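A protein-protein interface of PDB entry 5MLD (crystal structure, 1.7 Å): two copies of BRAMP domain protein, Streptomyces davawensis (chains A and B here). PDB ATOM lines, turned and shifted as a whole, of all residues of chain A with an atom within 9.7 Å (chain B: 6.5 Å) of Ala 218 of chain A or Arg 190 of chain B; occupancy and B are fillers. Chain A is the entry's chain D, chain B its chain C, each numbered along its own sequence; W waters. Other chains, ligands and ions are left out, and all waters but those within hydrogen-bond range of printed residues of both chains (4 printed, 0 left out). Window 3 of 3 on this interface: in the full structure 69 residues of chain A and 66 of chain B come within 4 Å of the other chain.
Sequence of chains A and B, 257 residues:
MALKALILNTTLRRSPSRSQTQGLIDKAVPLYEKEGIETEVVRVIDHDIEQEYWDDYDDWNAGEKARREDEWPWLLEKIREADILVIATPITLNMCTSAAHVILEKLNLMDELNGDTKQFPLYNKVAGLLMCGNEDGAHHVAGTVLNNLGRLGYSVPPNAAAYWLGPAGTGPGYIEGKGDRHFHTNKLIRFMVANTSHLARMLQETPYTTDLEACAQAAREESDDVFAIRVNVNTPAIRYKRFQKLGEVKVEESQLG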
ATOM      1  N   TYR A 123      11.619  -6.202 -29.940  1.00  0.00           N
ATOM      2  CA  TYR A 123      10.400  -5.975 -29.177  1.00  0.00           C
ATOM      3  C   TYR A 123       9.447  -5.049 -29.930  1.00  0.00           C
ATOM      4  O   TYR A 123       9.868  -4.170 -30.689  1.00  0.00           O
ATOM      5  CB  TYR A 123      10.734  -5.380 -27.805  1.00  0.00           C
ATOM      6  CG  TYR A 123      10.499  -6.362 -26.686  1.00  0.00           C
ATOM      7  CD1 TYR A 123      11.254  -7.531 -26.599  1.00  0.00           C
ATOM      8  CD2 TYR A 123       9.514  -6.143 -25.734  1.00  0.00           C
ATOM      9  CE1 TYR A 123      11.036  -8.441 -25.593  1.00  0.00           C
ATOM     10  CE2 TYR A 123       9.286  -7.050 -24.726  1.00  0.00           C
ATOM     11  CZ  TYR A 123      10.048  -8.201 -24.657  1.00  0.00           C
ATOM     12  OH  TYR A 123       9.820  -9.102 -23.647  1.00  0.00           O
ATOM     13  N   THR A 210       7.562  -2.964 -20.585  1.00  0.00           N
ATOM     14  CA  THR A 210       8.352  -3.843 -19.740  1.00  0.00           C
ATOM     15  C   THR A 210       9.819  -3.440 -19.758  1.00  0.00           C
ATOM     16  O   THR A 210      10.415  -3.228 -20.818  1.00  0.00           O
ATOM     17  CB  THR A 210       8.205  -5.292 -20.207  1.00  0.00           C
ATOM     18  OG1 THR A 210       6.822  -5.590 -20.398  1.00  0.00           O
ATOM     19  CG2 THR A 210       8.776  -6.248 -19.154  1.00  0.00           C
ATOM     20  N   ASP A 211      10.385  -3.307 -18.569  1.00  0.00           N
ATOM     21  CA  ASP A 211      11.814  -3.112 -18.379  1.00  0.00           C
ATOM     22  C   ASP A 211      12.386  -4.495 -18.075  1.00  0.00           C
ATOM     23  O   ASP A 211      12.261  -4.990 -16.953  1.00  0.00           O
ATOM     24  CB  ASP A 211      12.059  -2.122 -17.243  1.00  0.00           C
ATOM     25  CG  ASP A 211      13.523  -1.763 -17.072  1.00  0.00           C
ATOM     26  OD1 ASP A 211      14.403  -2.572 -17.444  1.00  0.00           O
ATOM     27  OD2 ASP A 211      13.795  -0.661 -16.542  1.00  0.00           O
ATOM     28  N   LEU A 212      12.982  -5.139 -19.087  1.00  0.00           N
ATOM     29  CA  LEU A 212      13.543  -6.473 -18.868  1.00  0.00           C
ATOM     30  C   LEU A 212      14.673  -6.434 -17.845  1.00  0.00           C
ATOM     31  O   LEU A 212      14.837  -7.363 -17.046  1.00  0.00           O
ATOM     32  CB  LEU A 212      14.040  -7.061 -20.191  1.00  0.00           C
ATOM     33  CG  LEU A 212      12.963  -7.180 -21.278  1.00  0.00           C
ATOM     34  CD1 LEU A 212      13.542  -7.779 -22.553  1.00  0.00           C
ATOM     35  CD2 LEU A 212      11.768  -7.982 -20.783  1.00  0.00           C
ATOM     36  N   GLU A 213      15.473  -5.370 -17.870  1.00  0.00           N
ATOM     37  CA  GLU A 213      16.575  -5.236 -16.923  1.00  0.00           C
ATOM     38  C   GLU A 213      16.065  -5.166 -15.486  1.00  0.00           C
ATOM     39  O   GLU A 213      16.610  -5.823 -14.591  1.00  0.00           O
ATOM     40  CB  GLU A 213      17.385  -4.000 -17.296  1.00  0.00           C
ATOM     41  CG  GLU A 213      18.546  -3.642 -16.411  1.00  0.00           C
ATOM     42  CD  GLU A 213      19.198  -2.363 -16.898  1.00  0.00           C
ATOM     43  OE1 GLU A 213      20.090  -2.436 -17.773  1.00  0.00           O
ATOM     44  OE2 GLU A 213      18.773  -1.278 -16.442  1.00  0.00           O
ATOM     45  N   ALA A 214      15.013  -4.374 -15.249  1.00  0.00           N
ATOM     46  CA  ALA A 214      14.393  -4.319 -13.926  1.00  0.00           C
ATOM     47  C   ALA A 214      13.823  -5.670 -13.512  1.00  0.00           C
ATOM     48  O   ALA A 214      13.976  -6.088 -12.361  1.00  0.00           O
ATOM     49  CB  ALA A 214      13.296  -3.254 -13.909  1.00  0.00           C
ATOM     50  N   CYS A 215      13.140  -6.359 -14.432  1.00  0.00           N
ATOM     51  CA  CYS A 215      12.651  -7.701 -14.133  1.00  0.00           C
ATOM     52  C   CYS A 215      13.798  -8.625 -13.746  1.00  0.00           C
ATOM     53  O   CYS A 215      13.698  -9.373 -12.768  1.00  0.00           O
ATOM     54  CB  CYS A 215      11.895  -8.269 -15.338  1.00  0.00           C
ATOM     55  SG  CYS A 215      10.281  -7.533 -15.666  1.00  0.00           S
ATOM     56  N   ALA A 216      14.911  -8.561 -14.484  1.00  0.00           N
ATOM     57  CA  ALA A 216      16.038  -9.433 -14.169  1.00  0.00           C
ATOM     58  C   ALA A 216      16.648  -9.067 -12.826  1.00  0.00           C
ATOM     59  O   ALA A 216      17.023  -9.949 -12.047  1.00  0.00           O
ATOM     60  CB  ALA A 216      17.087  -9.379 -15.283  1.00  0.00           C
ATOM     61  N   GLN A 217      16.709  -7.770 -12.518  1.00  0.00           N
ATOM     62  CA  GLN A 217      17.229  -7.357 -11.220  1.00  0.00           C
ATOM     63  C   GLN A 217      16.351  -7.879 -10.089  1.00  0.00           C
ATOM     64  O   GLN A 217      16.863  -8.360  -9.074  1.00  0.00           O
ATOM     65  CB  GLN A 217      17.361  -5.837 -11.170  1.00  0.00           C
ATOM     66  CG  GLN A 217      18.582  -5.310 -11.941  1.00  0.00           C
ATOM     67  CD  GLN A 217      18.484  -3.830 -12.253  1.00  0.00           C
ATOM     68  OE1 GLN A 217      17.403  -3.239 -12.179  1.00  0.00           O
ATOM     69  NE2 GLN A 217      19.611  -3.223 -12.609  1.00  0.00           N
ATOM     70  N   ALA A 218      15.027  -7.819 -10.253  1.00  0.00           N
ATOM     71  CA  ALA A 218      14.154  -8.357  -9.215  1.00  0.00           C
ATOM     72  C   ALA A 218      14.311  -9.866  -9.091  1.00  0.00           C
ATOM     73  O   ALA A 218      14.241 -10.413  -7.987  1.00  0.00           O
ATOM     74  CB  ALA A 218      12.700  -7.984  -9.494  1.00  0.00           C
ATOM     75  N   ALA A 219      14.528 -10.558 -10.215  1.00  0.00           N
ATOM     76  CA  ALA A 219      14.761 -11.998 -10.161  1.00  0.00           C
ATOM     77  C   ALA A 219      16.079 -12.308  -9.458  1.00  0.00           C
ATOM     78  O   ALA A 219      16.169 -13.258  -8.668  1.00  0.00           O
ATOM     79  CB  ALA A 219      14.747 -12.577 -11.580  1.00  0.00           C
ATOM     80  N   ARG A 220      17.103 -11.497  -9.719  1.00  0.00           N
ATOM     81  CA  ARG A 220      18.389 -11.670  -9.057  1.00  0.00           C
ATOM     82  C   ARG A 220      18.245 -11.643  -7.533  1.00  0.00           C
ATOM     83  O   ARG A 220      18.893 -12.426  -6.832  1.00  0.00           O
ATOM     84  CB  ARG A 220      19.354 -10.589  -9.541  1.00  0.00           C
ATOM     85  CG  ARG A 220      20.672 -10.555  -8.798  1.00  0.00           C
ATOM     86  CD  ARG A 220      21.432  -9.282  -9.094  1.00  0.00           C
ATOM     87  NE  ARG A 220      22.847  -9.591  -9.166  1.00  0.00           N
ATOM     88  CZ  ARG A 220      23.671  -9.668  -8.131  1.00  0.00           C
ATOM     89  NH1 ARG A 220      24.946  -9.959  -8.339  1.00  0.00           N
ATOM     90  NH2 ARG A 220      23.237  -9.364  -6.903  1.00  0.00           N
ATOM     91  N   GLU A 221      17.349 -10.799  -7.005  1.00  0.00           N
ATOM     92  CA  GLU A 221      17.236 -10.663  -5.552  1.00  0.00           C
ATOM     93  C   GLU A 221      16.615 -11.888  -4.893  1.00  0.00           C
ATOM     94  O   GLU A 221      16.866 -12.139  -3.708  1.00  0.00           O
ATOM     95  CB  GLU A 221      16.422  -9.416  -5.193  1.00  0.00           C
ATOM     96  CG  GLU A 221      17.043  -8.123  -5.706  1.00  0.00           C
ATOM     97  CD  GLU A 221      18.458  -7.900  -5.196  1.00  0.00           C
ATOM     98  OE1 GLU A 221      18.612  -7.649  -3.983  1.00  0.00           O
ATOM     99  OE2 GLU A 221      19.420  -7.964  -6.003  1.00  0.00           O
ATOM    100  N   GLU A 222      15.811 -12.657  -5.629  1.00  0.00           N
ATOM    101  CA  GLU A 222      15.109 -13.815  -5.093  1.00  0.00           C
ATOM    102  C   GLU A 222      15.746 -15.145  -5.505  1.00  0.00           C
ATOM    103  O   GLU A 222      15.113 -16.194  -5.351  1.00  0.00           O
ATOM    104  CB  GLU A 222      13.649 -13.788  -5.553  1.00  0.00           C
ATOM    105  CG  GLU A 222      13.516 -13.888  -7.082  1.00  0.00           C
ATOM    106  CD  GLU A 222      12.117 -13.602  -7.601  1.00  0.00           C
ATOM    107  OE1 GLU A 222      11.176 -13.500  -6.785  1.00  0.00           O
ATOM    108  OE2 GLU A 222      11.960 -13.480  -8.841  1.00  0.00           O
ATOM    109  N   SER A 223      16.969 -15.128  -6.026  1.00  0.00           N
ATOM    110  CA  SER A 223      17.541 -16.296  -6.683  1.00  0.00           C
ATOM    111  C   SER A 223      18.981 -16.527  -6.246  1.00  0.00           C
ATOM    112  O   SER A 223      19.646 -15.632  -5.716  1.00  0.00           O
ATOM    113  CB  SER A 223      17.491 -16.141  -8.209  1.00  0.00           C
ATOM    114  OG  SER A 223      16.167 -15.881  -8.654  1.00  0.00           O
ATOM    115  N   ASP A 224      19.456 -17.748  -6.502  1.00  0.00           N
ATOM    116  CA  ASP A 224      20.839 -18.148  -6.278  1.00  0.00           C
ATOM    117  C   ASP A 224      21.663 -17.897  -7.534  1.00  0.00           C
ATOM    118  O   ASP A 224      21.136 -17.882  -8.651  1.00  0.00           O
ATOM    119  CB  ASP A 224      20.929 -19.633  -5.911  1.00  0.00           C
ATOM    120  CG  ASP A 224      20.212 -19.974  -4.614  1.00  0.00           C
ATOM    121  OD1 ASP A 224      20.140 -19.106  -3.719  1.00  0.00           O
ATOM    122  OD2 ASP A 224      19.724 -21.121  -4.496  1.00  0.00           O
ATOM    123  N   LEU B  31       2.598 -11.683  -8.683  1.00  0.00           N
ATOM    124  CA  LEU B  31       2.988 -10.722  -9.710  1.00  0.00           C
ATOM    125  C   LEU B  31       1.775 -10.215 -10.480  1.00  0.00           C
ATOM    126  O   LEU B  31       1.661  -9.013 -10.753  1.00  0.00           O
ATOM    127  CB  LEU B  31       3.996 -11.350 -10.668  1.00  0.00           C
ATOM    128  CG  LEU B  31       5.324 -11.751 -10.032  1.00  0.00           C
ATOM    129  CD1 LEU B  31       6.169 -12.518 -11.032  1.00  0.00           C
ATOM    130  CD2 LEU B  31       6.060 -10.531  -9.512  1.00  0.00           C
ATOM    131  N   ALA B 162       7.423 -19.438 -19.532  1.00  0.00           N
ATOM    132  CA  ALA B 162       8.425 -19.544 -18.484  1.00  0.00           C
ATOM    133  C   ALA B 162       8.468 -20.979 -17.985  1.00  0.00           C
ATOM    134  O   ALA B 162       7.443 -21.672 -17.946  1.00  0.00           O
ATOM    135  CB  ALA B 162       8.118 -18.583 -17.330  1.00  0.00           C
ATOM    136  N   PHE B 183      17.455 -18.427 -10.999  1.00  0.00           N
ATOM    137  CA  PHE B 183      17.401 -17.090 -11.595  1.00  0.00           C
ATOM    138  C   PHE B 183      16.700 -17.083 -12.948  1.00  0.00           C
ATOM    139  O   PHE B 183      15.809 -16.262 -13.196  1.00  0.00           O
ATOM    140  CB  PHE B 183      18.818 -16.525 -11.745  1.00  0.00           C
ATOM    141  CG  PHE B 183      18.877 -15.231 -12.534  1.00  0.00           C
ATOM    142  CD1 PHE B 183      18.386 -14.044 -11.991  1.00  0.00           C
ATOM    143  CD2 PHE B 183      19.412 -15.206 -13.809  1.00  0.00           C
ATOM    144  CE1 PHE B 183      18.441 -12.858 -12.701  1.00  0.00           C
ATOM    145  CE2 PHE B 183      19.469 -14.031 -14.543  1.00  0.00           C
ATOM    146  CZ  PHE B 183      18.982 -12.840 -13.985  1.00  0.00           C
ATOM    147  N   THR B 185      14.531 -19.082 -14.361  1.00  0.00           N
ATOM    148  CA  THR B 185      13.092 -19.309 -14.276  1.00  0.00           C
ATOM    149  C   THR B 185      12.394 -18.092 -13.687  1.00  0.00           C
ATOM    150  O   THR B 185      11.352 -17.650 -14.189  1.00  0.00           O
ATOM    151  CB  THR B 185      12.813 -20.543 -13.429  1.00  0.00           C
ATOM    152  OG1 THR B 185      13.434 -21.684 -14.036  1.00  0.00           O
ATOM    153  CG2 THR B 185      11.318 -20.785 -13.299  1.00  0.00           C
ATOM    154  N   ASN B 186      12.976 -17.521 -12.632  1.00  0.00           N
ATOM    155  CA  ASN B 186      12.335 -16.399 -11.964  1.00  0.00           C
ATOM    156  C   ASN B 186      12.256 -15.173 -12.862  1.00  0.00           C
ATOM    157  O   ASN B 186      11.262 -14.429 -12.805  1.00  0.00           O
ATOM    158  CB  ASN B 186      13.075 -16.086 -10.667  1.00  0.00           C
ATOM    159  CG  ASN B 186      12.706 -17.043  -9.559  1.00  0.00           C
ATOM    160  OD1 ASN B 186      11.560 -17.479  -9.456  1.00  0.00           O
ATOM    161  ND2 ASN B 186      13.671 -17.378  -8.727  1.00  0.00           N
ATOM    162  N   LYS B 187      13.263 -14.953 -13.715  1.00  0.00           N
ATOM    163  CA  LYS B 187      13.173 -13.808 -14.612  1.00  0.00           C
ATOM    164  C   LYS B 187      12.208 -14.070 -15.768  1.00  0.00           C
ATOM    165  O   LYS B 187      11.486 -13.153 -16.179  1.00  0.00           O
ATOM    166  CB  LYS B 187      14.568 -13.395 -15.097  1.00  0.00           C
ATOM    167  CG  LYS B 187      15.104 -14.043 -16.364  1.00  0.00           C
ATOM    168  CD  LYS B 187      16.513 -13.475 -16.681  1.00  0.00           C
ATOM    169  CE  LYS B 187      17.042 -13.940 -18.026  1.00  0.00           C
ATOM    170  NZ  LYS B 187      18.511 -13.734 -18.114  1.00  0.00           N
ATOM    171  N   LEU B 188      12.133 -15.305 -16.279  1.00  0.00           N
ATOM    172  CA  LEU B 188      11.146 -15.585 -17.319  1.00  0.00           C
ATOM    173  C   LEU B 188       9.726 -15.405 -16.793  1.00  0.00           C
ATOM    174  O   LEU B 188       8.861 -14.870 -17.497  1.00  0.00           O
ATOM    175  CB  LEU B 188      11.329 -17.001 -17.864  1.00  0.00           C
ATOM    176  CG  LEU B 188      12.597 -17.231 -18.684  1.00  0.00           C
ATOM    177  CD1 LEU B 188      12.461 -18.499 -19.524  1.00  0.00           C
ATOM    178  CD2 LEU B 188      12.871 -16.050 -19.599  1.00  0.00           C
ATOM    179  N   ILE B 189       9.461 -15.858 -15.564  1.00  0.00           N
ATOM    180  CA  ILE B 189       8.130 -15.671 -14.990  1.00  0.00           C
ATOM    181  C   ILE B 189       7.798 -14.187 -14.899  1.00  0.00           C
ATOM    182  O   ILE B 189       6.683 -13.771 -15.213  1.00  0.00           O
ATOM    183  CB  ILE B 189       8.012 -16.366 -13.623  1.00  0.00           C
ATOM    184  CG1 ILE B 189       8.160 -17.874 -13.776  1.00  0.00           C
ATOM    185  CG2 ILE B 189       6.646 -16.067 -12.980  1.00  0.00           C
ATOM    186  CD1 ILE B 189       8.155 -18.622 -12.435  1.00  0.00           C
ATOM    187  N   ARG B 190       8.770 -13.363 -14.523  1.00  0.00           N
ATOM    188  CA  ARG B 190       8.512 -11.929 -14.470  1.00  0.00           C
ATOM    189  C   ARG B 190       8.264 -11.353 -15.862  1.00  0.00           C
ATOM    190  O   ARG B 190       7.387 -10.494 -16.029  1.00  0.00           O
ATOM    191  CB  ARG B 190       9.667 -11.220 -13.762  1.00  0.00           C
ATOM    192  CG  ARG B 190       9.700 -11.509 -12.272  1.00  0.00           C
ATOM    193  CD  ARG B 190      10.867 -10.833 -11.575  1.00  0.00           C
ATOM    194  NE  ARG B 190      10.795 -11.039 -10.134  1.00  0.00           N
ATOM    195  CZ  ARG B 190      10.090 -10.265  -9.313  1.00  0.00           C
ATOM    196  NH1 ARG B 190       9.422  -9.227  -9.805  1.00  0.00           N
ATOM    197  NH2 ARG B 190      10.059 -10.515  -8.007  1.00  0.00           N
ATOM    198  N   PHE B 191       9.010 -11.809 -16.882  1.00  0.00           N
ATOM    199  CA  PHE B 191       8.743 -11.346 -18.246  1.00  0.00           C
ATOM    200  C   PHE B 191       7.326 -11.715 -18.662  1.00  0.00           C
ATOM    201  O   PHE B 191       6.583 -10.888 -19.204  1.00  0.00           O
ATOM    202  CB  PHE B 191       9.719 -11.958 -19.259  1.00  0.00           C
ATOM    203  CG  PHE B 191      11.156 -11.550 -19.103  1.00  0.00           C
ATOM    204  CD1 PHE B 191      11.554 -10.613 -18.173  1.00  0.00           C
ATOM    205  CD2 PHE B 191      12.127 -12.142 -19.913  1.00  0.00           C
ATOM    206  CE1 PHE B 191      12.889 -10.259 -18.050  1.00  0.00           C
ATOM    207  CE2 PHE B 191      13.474 -11.794 -19.798  1.00  0.00           C
ATOM    208  CZ  PHE B 191      13.850 -10.848 -18.856  1.00  0.00           C
ATOM    209  N   MET B 192       6.954 -12.975 -18.423  1.00  0.00           N
ATOM    210  CA  MET B 192       5.649 -13.496 -18.811  1.00  0.00           C
ATOM    211  C   MET B 192       4.510 -12.674 -18.204  1.00  0.00           C
ATOM    212  O   MET B 192       3.584 -12.248 -18.911  1.00  0.00           O
ATOM    213  CB  MET B 192       5.559 -14.955 -18.365  1.00  0.00           C
ATOM    214  CG  MET B 192       4.471 -15.784 -18.992  1.00  0.00           C
ATOM    215  SD  MET B 192       2.916 -15.646 -18.100  1.00  0.00           S
ATOM    216  CE  MET B 192       3.364 -16.233 -16.466  1.00  0.00           C
ATOM    217  N   VAL B 193       4.540 -12.476 -16.888  1.00  0.00           N
ATOM    218  CA  VAL B 193       3.455 -11.751 -16.229  1.00  0.00           C
ATOM    219  C   VAL B 193       3.361 -10.328 -16.759  1.00  0.00           C
ATOM    220  O   VAL B 193       2.272  -9.832 -17.071  1.00  0.00           O
ATOM    221  CB  VAL B 193       3.642 -11.774 -14.704  1.00  0.00           C
ATOM    222  CG1 VAL B 193       2.632 -10.825 -14.027  1.00  0.00           C
ATOM    223  CG2 VAL B 193       3.479 -13.187 -14.191  1.00  0.00           C
ATOM    224  N   ALA B 194       4.499  -9.652 -16.877  1.00  0.00           N
ATOM    225  CA  ALA B 194       4.481  -8.265 -17.323  1.00  0.00           C
ATOM    226  C   ALA B 194       3.947  -8.144 -18.746  1.00  0.00           C
ATOM    227  O   ALA B 194       3.125  -7.268 -19.043  1.00  0.00           O
ATOM    228  CB  ALA B 194       5.883  -7.670 -17.214  1.00  0.00           C
ATOM    229  N   ASN B 195       4.386  -9.020 -19.639  1.00  0.00           N
ATOM    230  CA  ASN B 195       3.990  -8.884 -21.033  1.00  0.00           C
ATOM    231  C   ASN B 195       2.558  -9.342 -21.270  1.00  0.00           C
ATOM    232  O   ASN B 195       1.836  -8.708 -22.042  1.00  0.00           O
ATOM    233  CB  ASN B 195       4.949  -9.656 -21.933  1.00  0.00           C
ATOM    234  CG  ASN B 195       6.312  -9.023 -21.995  1.00  0.00           C
ATOM    235  OD1 ASN B 195       6.502  -7.887 -21.560  1.00  0.00           O
ATOM    236  ND2 ASN B 195       7.278  -9.748 -22.553  1.00  0.00           N
HETATM  237  O   HOH W   1       8.902  -8.111 -12.247  1.00  0.00           O
HETATM  238  O   HOH W   2      20.039 -19.425 -10.529  1.00  0.00           O
HETATM  239  O   HOH W   3       9.562 -15.108 -10.579  1.00  0.00           O
HETATM  240  O   HOH W   4       8.831 -13.562  -8.265  1.00  0.00           O
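The side-chain sulfur of Cys 215 of chain A sits at hydrogen-bond distance from the backbone carbonyl oxygen of Asp 211 of chain A (3.5 Å).
O of Ala 219 of chain A lies within hydrogen-bond range of OG of Ser 223 of chain A, 2.6 Å away.
Water W2 lies within hydrogen-bond range of O of Asp 224 of chain A (2.7 Å) and N of Phe 183 of chain B (2.8 Å).
Water W1 bridges NH1 of Arg 190 of chain B (2.7 Å) and SG of Cys 215 of chain A (3.7 Å).
Water W4 lies within hydrogen-bond range of OE1 of Glu 222 of chain A (2.8 Å) and NH2 of Arg 190 of chain B (3.3 Å).
Water W3 bridges the backbone carbonyl oxygen (O) of Asn 186 of chain B (2.9 Å) and the side-chain carboxylate (OE2) of Glu 222 of chain A (3.4 Å).
Ala 218 of chain A touches one residue of chain B.
Ala 162 of chain B touches none of the printed residues of chain A.
Printed residues of chain A within 4 Å of Asn 186 of chain B: Ala 219, Glu 222 and Ser 223.
Of the printed residues of chain A, Lys 187 of chain B touches Ala 219 (3.5 Å).
The nearest printed residue of chain A that does not touch Asn 195 of chain B is Leu 212 of chain A (5.1 Å).
Hydrophobic or aromatic side chains of chain A that line the printed part of chain B: Tyr 123, Leu 212, Ala 218 and Ala 219.
Among the printed residues, merely in contact across the chains: Thr 210 of chain A with Ala 194 of chain B (3.8 Å), Leu 212 of chain A with Phe 191 of chain B (3.6 Å), Cys 215 of chain A with Arg 190 of chain B (3.4 Å), Cys 215 of chain A with Phe 191 of chain B (3.5 Å), Ala 216 of chain A with Phe 183 of chain B (3.3 Å), Ala 218 of chain A with Arg 190 of chain B (3.5 Å), Ala 219 of chain A with Phe 183 of chain B (3.8 Å), Ala 219 of chain A with Asn 186 of chain B (3.8 Å), Ala 219 of chain A with Lys 187 of chain B (3.5 Å), Ala 219 of chain A with Arg 190 of chain B (3.8 Å), Arg 220 of chain A with Phe 183 of chain B (3.5 Å), Glu 222 of chain A with Asn 186 of chain B (3.4 Å) and Ser 223 of chain A with Phe 183 of chain B (3.4 Å).
No position is printed for both chains.
ND2 of Asn 186 of chain B lies within hydrogen-bond range of OG of Ser 223 of chain A (2.9 Å).
OE2 of Glu 222 of chain A lies within salt-bridge range of NE of Arg 190 of chain B, 3.0 Å away.
The side-chain amide nitrogen (ND2) of Asn 195 of chain B lies within hydrogen-bond range of the side-chain hydroxyl (OH) of Tyr 123 of chain A, at 2.8 Å.
OG1 of Thr 210 of chain A lies within hydrogen-bond range of OD1 of Asn 195 of chain B (2.6 Å).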
